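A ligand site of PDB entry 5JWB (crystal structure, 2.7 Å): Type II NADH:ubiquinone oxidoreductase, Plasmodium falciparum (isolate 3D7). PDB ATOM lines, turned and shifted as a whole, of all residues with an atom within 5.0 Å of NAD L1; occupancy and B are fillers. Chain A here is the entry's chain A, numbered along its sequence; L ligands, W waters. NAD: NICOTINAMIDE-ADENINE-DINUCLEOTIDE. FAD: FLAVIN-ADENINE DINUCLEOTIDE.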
ATOM      1  N   PHE A 143      17.973  22.013   7.366  1.00  0.00           N
ATOM      2  CA  PHE A 143      16.952  22.447   8.323  1.00  0.00           C
ATOM      3  C   PHE A 143      17.268  23.807   8.950  1.00  0.00           C
ATOM      4  O   PHE A 143      16.799  24.094  10.049  1.00  0.00           O
ATOM      5  CB  PHE A 143      16.778  21.416   9.438  1.00  0.00           C
ATOM      6  CG  PHE A 143      16.451  20.046   8.931  1.00  0.00           C
ATOM      7  CD1 PHE A 143      15.186  19.758   8.454  1.00  0.00           C
ATOM      8  CD2 PHE A 143      17.431  19.061   8.903  1.00  0.00           C
ATOM      9  CE1 PHE A 143      14.894  18.500   7.964  1.00  0.00           C
ATOM     10  CE2 PHE A 143      17.140  17.793   8.409  1.00  0.00           C
ATOM     11  CZ  PHE A 143      15.875  17.514   7.936  1.00  0.00           C
ATOM     12  N   ILE A 145      19.674  24.745  10.414  1.00  0.00           N
ATOM     13  CA  ILE A 145      20.516  24.588  11.600  1.00  0.00           C
ATOM     14  C   ILE A 145      21.848  25.302  11.425  1.00  0.00           C
ATOM     15  O   ILE A 145      22.495  25.195  10.373  1.00  0.00           O
ATOM     16  CB  ILE A 145      20.765  23.094  11.910  1.00  0.00           C
ATOM     17  CG1 ILE A 145      19.449  22.404  12.265  1.00  0.00           C
ATOM     18  CG2 ILE A 145      21.730  22.946  13.050  1.00  0.00           C
ATOM     19  CD1 ILE A 145      19.531  20.910  12.405  1.00  0.00           C
ATOM     20  N   VAL A 194      25.008  11.916  10.664  1.00  0.00           N
ATOM     21  CA  VAL A 194      23.644  12.295  10.948  1.00  0.00           C
ATOM     22  C   VAL A 194      22.703  11.777   9.875  1.00  0.00           C
ATOM     23  O   VAL A 194      22.822  12.141   8.726  1.00  0.00           O
ATOM     24  CB  VAL A 194      23.494  13.814  11.069  1.00  0.00           C
ATOM     25  CG1 VAL A 194      22.060  14.162  11.406  1.00  0.00           C
ATOM     26  CG2 VAL A 194      24.432  14.337  12.129  1.00  0.00           C
ATOM     27  N   GLY A 195      21.776  10.918  10.262  1.00  0.00           N
ATOM     28  CA  GLY A 195      20.867  10.311   9.327  1.00  0.00           C
ATOM     29  C   GLY A 195      20.953   8.800   9.423  1.00  0.00           C
ATOM     30  O   GLY A 195      22.013   8.219   9.210  1.00  0.00           O
ATOM     31  N   GLY A 196      19.829   8.167   9.752  1.00  0.00           N
ATOM     32  CA  GLY A 196      19.774   6.722   9.802  1.00  0.00           C
ATOM     33  C   GLY A 196      18.997   6.153   8.640  1.00  0.00           C
ATOM     34  O   GLY A 196      18.517   5.024   8.684  1.00  0.00           O
ATOM     35  N   GLY A 197      18.851   6.947   7.572  1.00  0.00           N
ATOM     36  CA  GLY A 197      18.368   6.408   6.321  1.00  0.00           C
ATOM     37  C   GLY A 197      19.445   5.559   5.653  1.00  0.00           C
ATOM     38  O   GLY A 197      20.550   5.387   6.165  1.00  0.00           O
ATOM     39  N   PRO A 198      19.129   5.020   4.480  1.00  0.00           N
ATOM     40  CA  PRO A 198      20.107   4.159   3.808  1.00  0.00           C
ATOM     41  C   PRO A 198      21.449   4.861   3.544  1.00  0.00           C
ATOM     42  O   PRO A 198      22.479   4.205   3.702  1.00  0.00           O
ATOM     43  CB  PRO A 198      19.408   3.794   2.491  1.00  0.00           C
ATOM     44  CG  PRO A 198      17.977   4.139   2.684  1.00  0.00           C
ATOM     45  CD  PRO A 198      17.935   5.264   3.658  1.00  0.00           C
ATOM     46  N   THR A 199      21.451   6.133   3.164  1.00  0.00           N
ATOM     47  CA  THR A 199      22.711   6.853   2.934  1.00  0.00           C
ATOM     48  C   THR A 199      23.600   6.872   4.195  1.00  0.00           C
ATOM     49  O   THR A 199      24.726   6.359   4.190  1.00  0.00           O
ATOM     50  CB  THR A 199      22.489   8.319   2.490  1.00  0.00           C
ATOM     51  OG1 THR A 199      21.819   8.347   1.233  1.00  0.00           O
ATOM     52  CG2 THR A 199      23.825   9.015   2.338  1.00  0.00           C
ATOM     53  N   GLY A 200      23.081   7.484   5.268  1.00  0.00           N
ATOM     54  CA  GLY A 200      23.767   7.490   6.550  1.00  0.00           C
ATOM     55  C   GLY A 200      24.230   6.111   6.978  1.00  0.00           C
ATOM     56  O   GLY A 200      25.379   5.931   7.391  1.00  0.00           O
ATOM     57  N   GLU A 202      24.749   3.335   5.153  1.00  0.00           N
ATOM     58  CA  GLU A 202      25.778   2.774   4.288  1.00  0.00           C
ATOM     59  C   GLU A 202      27.126   3.467   4.487  1.00  0.00           C
ATOM     60  O   GLU A 202      28.166   2.808   4.560  1.00  0.00           O
ATOM     61  CB  GLU A 202      25.322   2.827   2.824  1.00  0.00           C
ATOM     62  CG  GLU A 202      24.113   1.910   2.519  1.00  0.00           C
ATOM     63  CD  GLU A 202      23.646   1.901   1.051  1.00  0.00           C
ATOM     64  OE1 GLU A 202      23.807   2.907   0.315  1.00  0.00           O
ATOM     65  OE2 GLU A 202      23.104   0.865   0.630  1.00  0.00           O
ATOM     66  N   ILE A 231      23.548   9.031  14.151  1.00  0.00           N
ATOM     67  CA  ILE A 231      22.488   9.686  14.894  1.00  0.00           C
ATOM     68  C   ILE A 231      21.236   9.741  14.064  1.00  0.00           C
ATOM     69  O   ILE A 231      21.265  10.155  12.916  1.00  0.00           O
ATOM     70  CB  ILE A 231      22.854  11.117  15.348  1.00  0.00           C
ATOM     71  CG1 ILE A 231      24.018  11.102  16.335  1.00  0.00           C
ATOM     72  CG2 ILE A 231      21.654  11.803  16.019  1.00  0.00           C
ATOM     73  CD1 ILE A 231      25.364  11.097  15.696  1.00  0.00           C
ATOM     74  N   GLU A 232      20.125   9.312  14.662  1.00  0.00           N
ATOM     75  CA  GLU A 232      18.850   9.236  13.964  1.00  0.00           C
ATOM     76  C   GLU A 232      17.689   9.666  14.890  1.00  0.00           C
ATOM     77  O   GLU A 232      17.612   9.208  16.038  1.00  0.00           O
ATOM     78  CB  GLU A 232      18.650   7.819  13.421  1.00  0.00           C
ATOM     79  CG  GLU A 232      17.210   7.464  13.154  1.00  0.00           C
ATOM     80  CD  GLU A 232      16.612   8.327  12.060  1.00  0.00           C
ATOM     81  OE1 GLU A 232      17.378   8.676  11.136  1.00  0.00           O
ATOM     82  OE2 GLU A 232      15.417   8.681  12.151  1.00  0.00           O
ATOM     83  N   GLY A 233      16.813  10.545  14.405  1.00  0.00           N
ATOM     84  CA  GLY A 233      15.687  11.015  15.187  1.00  0.00           C
ATOM     85  C   GLY A 233      14.690   9.936  15.624  1.00  0.00           C
ATOM     86  O   GLY A 233      14.209   9.950  16.747  1.00  0.00           O
ATOM     87  N   GLY A 234      14.378   9.004  14.734  1.00  0.00           N
ATOM     88  CA  GLY A 234      13.436   7.953  15.066  1.00  0.00           C
ATOM     89  C   GLY A 234      14.077   6.774  15.759  1.00  0.00           C
ATOM     90  O   GLY A 234      15.274   6.784  16.055  1.00  0.00           O
ATOM     91  N   PRO A 239      14.420   3.146   8.643  1.00  0.00           N
ATOM     92  CA  PRO A 239      13.019   3.074   9.038  1.00  0.00           C
ATOM     93  C   PRO A 239      12.131   2.668   7.888  1.00  0.00           C
ATOM     94  O   PRO A 239      11.121   2.014   8.101  1.00  0.00           O
ATOM     95  CB  PRO A 239      12.697   4.499   9.479  1.00  0.00           C
ATOM     96  CG  PRO A 239      13.667   5.344   8.764  1.00  0.00           C
ATOM     97  CD  PRO A 239      14.920   4.530   8.630  1.00  0.00           C
ATOM     98  N   PHE A 241      12.526   0.567   5.685  1.00  0.00           N
ATOM     99  CA  PHE A 241      12.735  -0.803   5.228  1.00  0.00           C
ATOM    100  C   PHE A 241      11.720  -1.780   5.861  1.00  0.00           C
ATOM    101  O   PHE A 241      10.591  -1.928   5.357  1.00  0.00           O
ATOM    102  CB  PHE A 241      14.161  -1.270   5.516  1.00  0.00           C
ATOM    103  CG  PHE A 241      15.146  -0.909   4.424  1.00  0.00           C
ATOM    104  CD1 PHE A 241      15.746  -1.880   3.639  1.00  0.00           C
ATOM    105  CD2 PHE A 241      15.469   0.424   4.172  1.00  0.00           C
ATOM    106  CE1 PHE A 241      16.652  -1.541   2.636  1.00  0.00           C
ATOM    107  CE2 PHE A 241      16.389   0.774   3.170  1.00  0.00           C
ATOM    108  CZ  PHE A 241      16.976  -0.213   2.397  1.00  0.00           C
ATOM    109  N   TYR A 264      17.548  10.441  18.674  1.00  0.00           N
ATOM    110  CA  TYR A 264      18.244  11.698  18.926  1.00  0.00           C
ATOM    111  C   TYR A 264      18.240  12.568  17.680  1.00  0.00           C
ATOM    112  O   TYR A 264      18.486  12.105  16.580  1.00  0.00           O
ATOM    113  CB  TYR A 264      19.689  11.462  19.379  1.00  0.00           C
ATOM    114  CG  TYR A 264      19.837  11.163  20.854  1.00  0.00           C
ATOM    115  CD1 TYR A 264      19.709  12.165  21.808  1.00  0.00           C
ATOM    116  CD2 TYR A 264      20.103   9.875  21.306  1.00  0.00           C
ATOM    117  CE1 TYR A 264      19.829  11.904  23.142  1.00  0.00           C
ATOM    118  CE2 TYR A 264      20.239   9.601  22.649  1.00  0.00           C
ATOM    119  CZ  TYR A 264      20.105  10.616  23.563  1.00  0.00           C
ATOM    120  OH  TYR A 264      20.232  10.344  24.899  1.00  0.00           O
ATOM    121  N   TYR A 265      17.939  13.846  17.872  1.00  0.00           N
ATOM    122  CA  TYR A 265      17.936  14.807  16.792  1.00  0.00           C
ATOM    123  C   TYR A 265      19.131  15.726  16.994  1.00  0.00           C
ATOM    124  O   TYR A 265      19.315  16.238  18.081  1.00  0.00           O
ATOM    125  CB  TYR A 265      16.618  15.605  16.750  1.00  0.00           C
ATOM    126  CG  TYR A 265      15.502  14.955  15.954  1.00  0.00           C
ATOM    127  CD1 TYR A 265      15.624  14.785  14.573  1.00  0.00           C
ATOM    128  CD2 TYR A 265      14.324  14.516  16.575  1.00  0.00           C
ATOM    129  CE1 TYR A 265      14.581  14.178  13.810  1.00  0.00           C
ATOM    130  CE2 TYR A 265      13.283  13.914  15.829  1.00  0.00           C
ATOM    131  CZ  TYR A 265      13.419  13.746  14.446  1.00  0.00           C
ATOM    132  OH  TYR A 265      12.416  13.149  13.718  1.00  0.00           O
ATOM    133  N   VAL A 266      19.928  15.943  15.967  1.00  0.00           N
ATOM    134  CA  VAL A 266      20.943  17.001  16.026  1.00  0.00           C
ATOM    135  C   VAL A 266      20.220  18.357  15.888  1.00  0.00           C
ATOM    136  O   VAL A 266      19.357  18.489  15.021  1.00  0.00           O
ATOM    137  CB  VAL A 266      22.027  16.816  14.931  1.00  0.00           C
ATOM    138  CG1 VAL A 266      22.885  18.042  14.822  1.00  0.00           C
ATOM    139  CG2 VAL A 266      22.878  15.575  15.238  1.00  0.00           C
ATOM    140  N   TRP A 295      26.658  14.839   7.115  1.00  0.00           N
ATOM    141  CA  TRP A 295      25.219  15.168   7.137  1.00  0.00           C
ATOM    142  C   TRP A 295      24.429  14.436   6.051  1.00  0.00           C
ATOM    143  O   TRP A 295      24.502  14.796   4.878  1.00  0.00           O
ATOM    144  CB  TRP A 295      24.990  16.664   6.976  1.00  0.00           C
ATOM    145  CG  TRP A 295      23.697  17.188   7.554  1.00  0.00           C
ATOM    146  CD1 TRP A 295      22.525  17.401   6.885  1.00  0.00           C
ATOM    147  CD2 TRP A 295      23.460  17.587   8.903  1.00  0.00           C
ATOM    148  NE1 TRP A 295      21.572  17.892   7.745  1.00  0.00           N
ATOM    149  CE2 TRP A 295      22.122  18.013   8.988  1.00  0.00           C
ATOM    150  CE3 TRP A 295      24.255  17.619  10.055  1.00  0.00           C
ATOM    151  CZ2 TRP A 295      21.566  18.469  10.173  1.00  0.00           C
ATOM    152  CZ3 TRP A 295      23.691  18.067  11.231  1.00  0.00           C
ATOM    153  CH2 TRP A 295      22.364  18.476  11.278  1.00  0.00           C
ATOM    154  N   ALA A 296      23.680  13.419   6.454  1.00  0.00           N
ATOM    155  CA  ALA A 296      22.914  12.619   5.507  1.00  0.00           C
ATOM    156  C   ALA A 296      21.434  12.588   5.868  1.00  0.00           C
ATOM    157  O   ALA A 296      20.829  11.532   5.933  1.00  0.00           O
ATOM    158  CB  ALA A 296      23.463  11.202   5.433  1.00  0.00           C
ATOM    159  N   SER A 297      20.856  13.753   6.118  1.00  0.00           N
ATOM    160  CA  SER A 297      19.418  13.856   6.337  1.00  0.00           C
ATOM    161  C   SER A 297      18.716  13.850   4.990  1.00  0.00           C
ATOM    162  O   SER A 297      19.337  13.548   3.952  1.00  0.00           O
ATOM    163  CB  SER A 297      19.072  15.129   7.099  1.00  0.00           C
ATOM    164  OG  SER A 297      19.357  16.277   6.301  1.00  0.00           O
ATOM    165  N   GLY A 298      17.431  14.181   4.989  1.00  0.00           N
ATOM    166  CA  GLY A 298      16.644  14.101   3.760  1.00  0.00           C
ATOM    167  C   GLY A 298      16.915  15.185   2.716  1.00  0.00           C
ATOM    168  O   GLY A 298      17.993  15.796   2.727  1.00  0.00           O
ATOM    169  N   LEU A 299      15.929  15.430   1.846  1.00  0.00           N
ATOM    170  CA  LEU A 299      16.093  16.318   0.685  1.00  0.00           C
ATOM    171  C   LEU A 299      15.508  17.711   0.855  1.00  0.00           C
ATOM    172  O   LEU A 299      14.722  17.960   1.758  1.00  0.00           O
ATOM    173  CB  LEU A 299      15.456  15.661  -0.544  1.00  0.00           C
ATOM    174  CG  LEU A 299      15.946  14.234  -0.747  1.00  0.00           C
ATOM    175  CD1 LEU A 299      15.176  13.556  -1.864  1.00  0.00           C
ATOM    176  CD2 LEU A 299      17.437  14.194  -1.021  1.00  0.00           C
ATOM    177  N   PRO A 422      11.489   9.427  -3.821  1.00  0.00           N
ATOM    178  CA  PRO A 422      12.651  10.025  -4.477  1.00  0.00           C
ATOM    179  C   PRO A 422      13.812   9.065  -4.471  1.00  0.00           C
ATOM    180  O   PRO A 422      14.689   9.114  -3.606  1.00  0.00           O
ATOM    181  CB  PRO A 422      12.934  11.266  -3.628  1.00  0.00           C
ATOM    182  CG  PRO A 422      12.456  10.895  -2.274  1.00  0.00           C
ATOM    183  CD  PRO A 422      11.289   9.987  -2.477  1.00  0.00           C
ATOM    184  N   THR A 423      13.781   8.157  -5.436  1.00  0.00           N
ATOM    185  CA  THR A 423      14.805   7.131  -5.590  1.00  0.00           C
ATOM    186  C   THR A 423      15.297   7.094  -7.016  1.00  0.00           C
ATOM    187  O   THR A 423      14.628   7.581  -7.945  1.00  0.00           O
ATOM    188  CB  THR A 423      14.262   5.744  -5.201  1.00  0.00           C
ATOM    189  OG1 THR A 423      13.313   5.301  -6.187  1.00  0.00           O
ATOM    190  CG2 THR A 423      13.630   5.787  -3.803  1.00  0.00           C
ATOM    191  N   SER A 460      14.625  -2.758  -2.310  1.00  0.00           N
ATOM    192  CA  SER A 460      15.760  -1.930  -1.910  1.00  0.00           C
ATOM    193  C   SER A 460      16.845  -2.748  -1.212  1.00  0.00           C
ATOM    194  O   SER A 460      16.528  -3.675  -0.477  1.00  0.00           O
ATOM    195  CB  SER A 460      15.310  -0.808  -0.994  1.00  0.00           C
ATOM    196  OG  SER A 460      14.276  -0.059  -1.610  1.00  0.00           O
ATOM    197  N   LEU A 461      18.105  -2.383  -1.425  1.00  0.00           N
ATOM    198  CA  LEU A 461      19.249  -3.057  -0.801  1.00  0.00           C
ATOM    199  C   LEU A 461      20.064  -2.078   0.026  1.00  0.00           C
ATOM    200  O   LEU A 461      19.994  -0.877  -0.185  1.00  0.00           O
ATOM    201  CB  LEU A 461      20.182  -3.681  -1.831  1.00  0.00           C
ATOM    202  CG  LEU A 461      19.790  -4.729  -2.853  1.00  0.00           C
ATOM    203  CD1 LEU A 461      19.016  -4.089  -3.993  1.00  0.00           C
ATOM    204  CD2 LEU A 461      21.049  -5.395  -3.391  1.00  0.00           C
ATOM    205  N   ALA A 462      20.877  -2.596   0.936  1.00  0.00           N
ATOM    206  CA  ALA A 462      21.732  -1.765   1.767  1.00  0.00           C
ATOM    207  C   ALA A 462      22.894  -2.564   2.294  1.00  0.00           C
ATOM    208  O   ALA A 462      22.704  -3.670   2.759  1.00  0.00           O
ATOM    209  CB  ALA A 462      20.945  -1.157   2.919  1.00  0.00           C
ATOM    210  N   TYR A 492      23.907  -5.220  -8.412  1.00  0.00           N
ATOM    211  CA  TYR A 492      24.444  -3.950  -8.862  1.00  0.00           C
ATOM    212  C   TYR A 492      25.321  -4.046 -10.113  1.00  0.00           C
ATOM    213  O   TYR A 492      25.405  -3.061 -10.852  1.00  0.00           O
ATOM    214  CB  TYR A 492      25.221  -3.254  -7.733  1.00  0.00           C
ATOM    215  CG  TYR A 492      24.318  -2.489  -6.774  1.00  0.00           C
ATOM    216  CD1 TYR A 492      23.644  -1.339  -7.200  1.00  0.00           C
ATOM    217  CD2 TYR A 492      24.124  -2.910  -5.466  1.00  0.00           C
ATOM    218  CE1 TYR A 492      22.810  -0.633  -6.339  1.00  0.00           C
ATOM    219  CE2 TYR A 492      23.292  -2.199  -4.589  1.00  0.00           C
ATOM    220  CZ  TYR A 492      22.631  -1.063  -5.036  1.00  0.00           C
ATOM    221  OH  TYR A 492      21.795  -0.352  -4.189  1.00  0.00           O
HETATM  222  PA  NAD L   1      16.253   9.775   4.411  1.00  0.00           P
HETATM  223  O1A NAD L   1      15.772   8.450   3.853  1.00  0.00           O
HETATM  224  O2A NAD L   1      15.130  10.774   4.450  1.00  0.00           O
HETATM  225  O5B NAD L   1      16.801   9.557   5.872  1.00  0.00           O
HETATM  226  C5B NAD L   1      17.114  10.673   6.658  1.00  0.00           C
HETATM  227  C4B NAD L   1      17.013  10.277   8.088  1.00  0.00           C
HETATM  228  O4B NAD L   1      17.725  11.237   8.932  1.00  0.00           O
HETATM  229  C3B NAD L   1      15.600  10.261   8.534  1.00  0.00           C
HETATM  230  O3B NAD L   1      15.329   8.929   9.064  1.00  0.00           O
HETATM  231  C2B NAD L   1      15.441  11.356   9.524  1.00  0.00           C
HETATM  232  O2B NAD L   1      14.574  10.971  10.634  1.00  0.00           O
HETATM  233  C1B NAD L   1      16.788  11.639  10.023  1.00  0.00           C
HETATM  234  N9A NAD L   1      17.071  12.980  10.392  1.00  0.00           N
HETATM  235  C8A NAD L   1      16.690  14.059   9.707  1.00  0.00           C
HETATM  236  N7A NAD L   1      17.162  15.219  10.316  1.00  0.00           N
HETATM  237  C5A NAD L   1      17.886  14.688  11.471  1.00  0.00           C
HETATM  238  C6A NAD L   1      18.589  15.254  12.508  1.00  0.00           C
HETATM  239  N6A NAD L   1      18.715  16.666  12.593  1.00  0.00           N
HETATM  240  N1A NAD L   1      19.163  14.469  13.465  1.00  0.00           N
HETATM  241  C2A NAD L   1      19.028  13.131  13.346  1.00  0.00           C
HETATM  242  N3A NAD L   1      18.344  12.435  12.383  1.00  0.00           N
HETATM  243  C4A NAD L   1      17.801  13.260  11.464  1.00  0.00           C
HETATM  244  O3  NAD L   1      17.446  10.357   3.496  1.00  0.00           O
HETATM  245  PN  NAD L   1      18.541   9.509   2.644  1.00  0.00           P
HETATM  246  O1N NAD L   1      19.191   8.371   3.372  1.00  0.00           O
HETATM  247  O2N NAD L   1      19.664  10.449   2.374  1.00  0.00           O
HETATM  248  O5D NAD L   1      17.869   8.942   1.300  1.00  0.00           O
HETATM  249  C5D NAD L   1      17.169   9.822   0.425  1.00  0.00           C
HETATM  250  C4D NAD L   1      16.513   9.049  -0.651  1.00  0.00           C
HETATM  251  O4D NAD L   1      17.517   8.232  -1.418  1.00  0.00           O
HETATM  252  C3D NAD L   1      15.572   8.094  -0.046  1.00  0.00           C
HETATM  253  O3D NAD L   1      14.330   8.189  -0.774  1.00  0.00           O
HETATM  254  C2D NAD L   1      16.191   6.751  -0.144  1.00  0.00           C
HETATM  255  O2D NAD L   1      15.235   5.672  -0.257  1.00  0.00           O
HETATM  256  C1D NAD L   1      17.088   6.802  -1.326  1.00  0.00           C
HETATM  257  N1N NAD L   1      18.187   5.977  -1.069  1.00  0.00           N
HETATM  258  C2N NAD L   1      18.125   4.590  -1.254  1.00  0.00           C
HETATM  259  C3N NAD L   1      19.255   3.776  -0.969  1.00  0.00           C
HETATM  260  C7N NAD L   1      19.233   2.260  -1.144  1.00  0.00           C
HETATM  261  O7N NAD L   1      18.329   1.691  -1.757  1.00  0.00           O
HETATM  262  N7N NAD L   1      20.316   1.547  -0.568  1.00  0.00           N
HETATM  263  C4N NAD L   1      20.489   4.372  -0.497  1.00  0.00           C
HETATM  264  C5N NAD L   1      20.454   5.782  -0.326  1.00  0.00           C
HETATM  265  C6N NAD L   1      19.344   6.512  -0.613  1.00  0.00           C
HETATM  266  PA  FAD L   2      20.129  13.631  -9.471  1.00  0.00           P
HETATM  267  O1A FAD L   2      20.640  14.244  -8.184  1.00  0.00           O
HETATM  268  O2A FAD L   2      20.505  12.197  -9.727  1.00  0.00           O
HETATM  269  O5B FAD L   2      20.477  14.566 -10.721  1.00  0.00           O
HETATM  270  C5B FAD L   2      20.309  15.953 -10.650  1.00  0.00           C
HETATM  271  C4B FAD L   2      21.178  16.541 -11.737  1.00  0.00           C
HETATM  272  O4B FAD L   2      20.780  17.877 -11.971  1.00  0.00           O
HETATM  273  C3B FAD L   2      22.655  16.569 -11.374  1.00  0.00           C
HETATM  274  O3B FAD L   2      23.407  16.183 -12.499  1.00  0.00           O
HETATM  275  C2B FAD L   2      22.945  18.028 -11.103  1.00  0.00           C
HETATM  276  O2B FAD L   2      24.248  18.351 -11.496  1.00  0.00           O
HETATM  277  C1B FAD L   2      21.922  18.696 -12.005  1.00  0.00           C
HETATM  278  N9A FAD L   2      21.542  20.050 -11.610  1.00  0.00           N
HETATM  279  C8A FAD L   2      21.365  20.604 -10.369  1.00  0.00           C
HETATM  280  N7A FAD L   2      20.974  21.892 -10.522  1.00  0.00           N
HETATM  281  C5A FAD L   2      20.913  22.154 -11.851  1.00  0.00           C
HETATM  282  C6A FAD L   2      20.592  23.284 -12.589  1.00  0.00           C
HETATM  283  N6A FAD L   2      19.893  24.276 -12.060  1.00  0.00           N
HETATM  284  N1A FAD L   2      20.631  23.200 -13.951  1.00  0.00           N
HETATM  285  C2A FAD L   2      20.964  22.025 -14.596  1.00  0.00           C
HETATM  286  N3A FAD L   2      21.282  20.909 -13.868  1.00  0.00           N
HETATM  287  C4A FAD L   2      21.261  20.991 -12.531  1.00  0.00           C
HETATM  288  N1  FAD L   2      18.110   5.602  -5.024  1.00  0.00           N
HETATM  289  C2  FAD L   2      17.737   4.306  -5.287  1.00  0.00           C
HETATM  290  O2  FAD L   2      16.677   4.068  -5.863  1.00  0.00           O
HETATM  291  N3  FAD L   2      18.556   3.266  -4.892  1.00  0.00           N
HETATM  292  C4  FAD L   2      19.748   3.493  -4.244  1.00  0.00           C
HETATM  293  O4  FAD L   2      20.469   2.540  -3.895  1.00  0.00           O
HETATM  294  C4X FAD L   2      20.127   4.792  -3.988  1.00  0.00           C
HETATM  295  N5  FAD L   2      21.315   5.047  -3.359  1.00  0.00           N
HETATM  296  C5X FAD L   2      21.691   6.360  -3.113  1.00  0.00           C
HETATM  297  C6  FAD L   2      22.879   6.648  -2.458  1.00  0.00           C
HETATM  298  C7  FAD L   2      23.249   7.968  -2.201  1.00  0.00           C
HETATM  299  C7M FAD L   2      24.558   8.247  -1.508  1.00  0.00           C
HETATM  300  C8  FAD L   2      22.408   8.999  -2.603  1.00  0.00           C
HETATM  301  C8M FAD L   2      22.747  10.436  -2.354  1.00  0.00           C
HETATM  302  C9  FAD L   2      21.220   8.719  -3.255  1.00  0.00           C
HETATM  303  C9A FAD L   2      20.851   7.405  -3.495  1.00  0.00           C
HETATM  304  N10 FAD L   2      19.648   7.144  -4.138  1.00  0.00           N
HETATM  305  C10 FAD L   2      19.300   5.843  -4.385  1.00  0.00           C
HETATM  306  C1' FAD L   2      18.749   8.263  -4.554  1.00  0.00           C
HETATM  307  C2' FAD L   2      19.003   8.732  -5.968  1.00  0.00           C
HETATM  308  O2' FAD L   2      20.310   9.203  -6.146  1.00  0.00           O
HETATM  309  C3' FAD L   2      18.096   9.910  -6.250  1.00  0.00           C
HETATM  310  O3' FAD L   2      16.764   9.528  -5.993  1.00  0.00           O
HETATM  311  C4' FAD L   2      18.303  10.241  -7.726  1.00  0.00           C
HETATM  312  O4' FAD L   2      19.489  11.003  -7.839  1.00  0.00           O
HETATM  313  C5' FAD L   2      17.160  11.018  -8.339  1.00  0.00           C
HETATM  314  O5' FAD L   2      17.620  11.384  -9.617  1.00  0.00           O
HETATM  315  P   FAD L   2      17.494  12.885 -10.185  1.00  0.00           P
HETATM  316  O1P FAD L   2      17.840  12.822 -11.643  1.00  0.00           O
HETATM  317  O2P FAD L   2      16.128  13.422  -9.870  1.00  0.00           O
HETATM  318  O3P FAD L   2      18.537  13.811  -9.398  1.00  0.00           O
HETATM  319  O   HOH W   1      17.118  11.041  -3.178  1.00  0.00           O
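The backbone carbonyl oxygen (O) of Leu 461 is in hydrogen-bond range of a nitrogen (N7N) of NAD L1 (2.5 Å).
The side-chain carboxylate of Glu 232 lies within hydrogen-bond range of an oxygen (O2B) of NAD L1 (2.9 Å).
O3D of NAD L1 sits at hydrogen-bond distance from O of Pro 422 (3.0 Å).
N1A of NAD L1 is in hydrogen-bond range of N of Val 266.
The backbone carbonyl oxygen (O) of Val 266 is in hydrogen-bond range of a nitrogen (N6A) of NAD L1, at 3.1 Å.
N7N of NAD L1 lies within hydrogen-bond range of OE2 of Glu 202 (3.1 Å).
The backbone NH (N) of Gly 233 lies within hydrogen-bond range of a nitrogen (N3A) of NAD L1.
O1N of NAD L1 sits at hydrogen-bond distance from N of Thr 199, at 3.2 Å.
The side-chain hydroxyl (OG1) of Thr 199 sits at hydrogen-bond distance from an oxygen (O2N) of NAD L1 (3.2 Å).
O3' of FAD L2 lies within hydrogen-bond range of O of Pro 422 (3.2 Å).
O3' of FAD L2 lies close to N of Thr 423, 3.3 Å away.
The backbone carbonyl oxygen (O) of Thr 423 lies close to an oxygen (O3') of FAD L2, at 3.5 Å.
An oxygen (O4) of FAD L2 is in hydrogen-bond range of the side-chain hydroxyl (OH) of Tyr 492 (3.2 Å).
O4 of FAD L2 sits close to N7N of NAD L1, at 3.5 Å.
The backbone carbonyl oxygen of Glu 232 sits at hydrogen-bond distance from the backbone NH of Tyr 264.
OE1 of Glu 232 lies within hydrogen-bond range of N of Gly 196 (2.9 Å).
The side-chain carboxylate (OE2) of Glu 232 sits at hydrogen-bond distance from the backbone NH (N) of Gly 234.
The backbone NH of Gly 233 sits at hydrogen-bond distance from the backbone carbonyl oxygen of Tyr 264, 3.2 Å away.
The backbone carbonyl oxygen (O) of Ile 231 is in hydrogen-bond range of the backbone NH (N) of Gly 195 (2.8 Å).
The indole nitrogen (NE1) of Trp 295 lies within hydrogen-bond range of the side-chain hydroxyl (OG) of Ser 297, at 3.1 Å.
The backbone carbonyl oxygen (O) of Val 194 lies within hydrogen-bond range of the backbone NH (N) of Ala 296, 2.7 Å away.
An oxygen (O2N) of NAD L1 lies close to the backbone carbonyl oxygen of Ser 297.
Residues that only touch NAD L1: Phe 143 (3.2 Å), Val 194 (3.6 Å), Gly 195 (3.3 Å), Gly 196 (3.8 Å), Gly 197 (3.5 Å), Pro 198 (3.2 Å), Ile 231 (3.7 Å), Pro 239 (3.96 Å), Tyr 264 (3.4 Å), Tyr 265 (3.6 Å), Ala 296 (3.9 Å), Gly 298 (3.7 Å), Thr 423 (3.9 Å) and Ser 460 (3.99 Å).
22 residues have an atom within 4 Å of NAD L1: Phe 143, Val 194, Gly 195, Gly 196, Gly 197, Pro 198, Thr 199, Glu 202, Ile 231, Glu 232, Gly 233, Pro 239, Tyr 264, Tyr 265, Val 266, Ala 296, Ser 297, Gly 298, Pro 422, Thr 423, Ser 460 and Leu 461.
Water W1 lies within hydrogen-bond range of O of Pro 422 (3.1 Å), O3' of FAD L2 (3.2 Å) and O4D of NAD L1 (3.3 Å).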
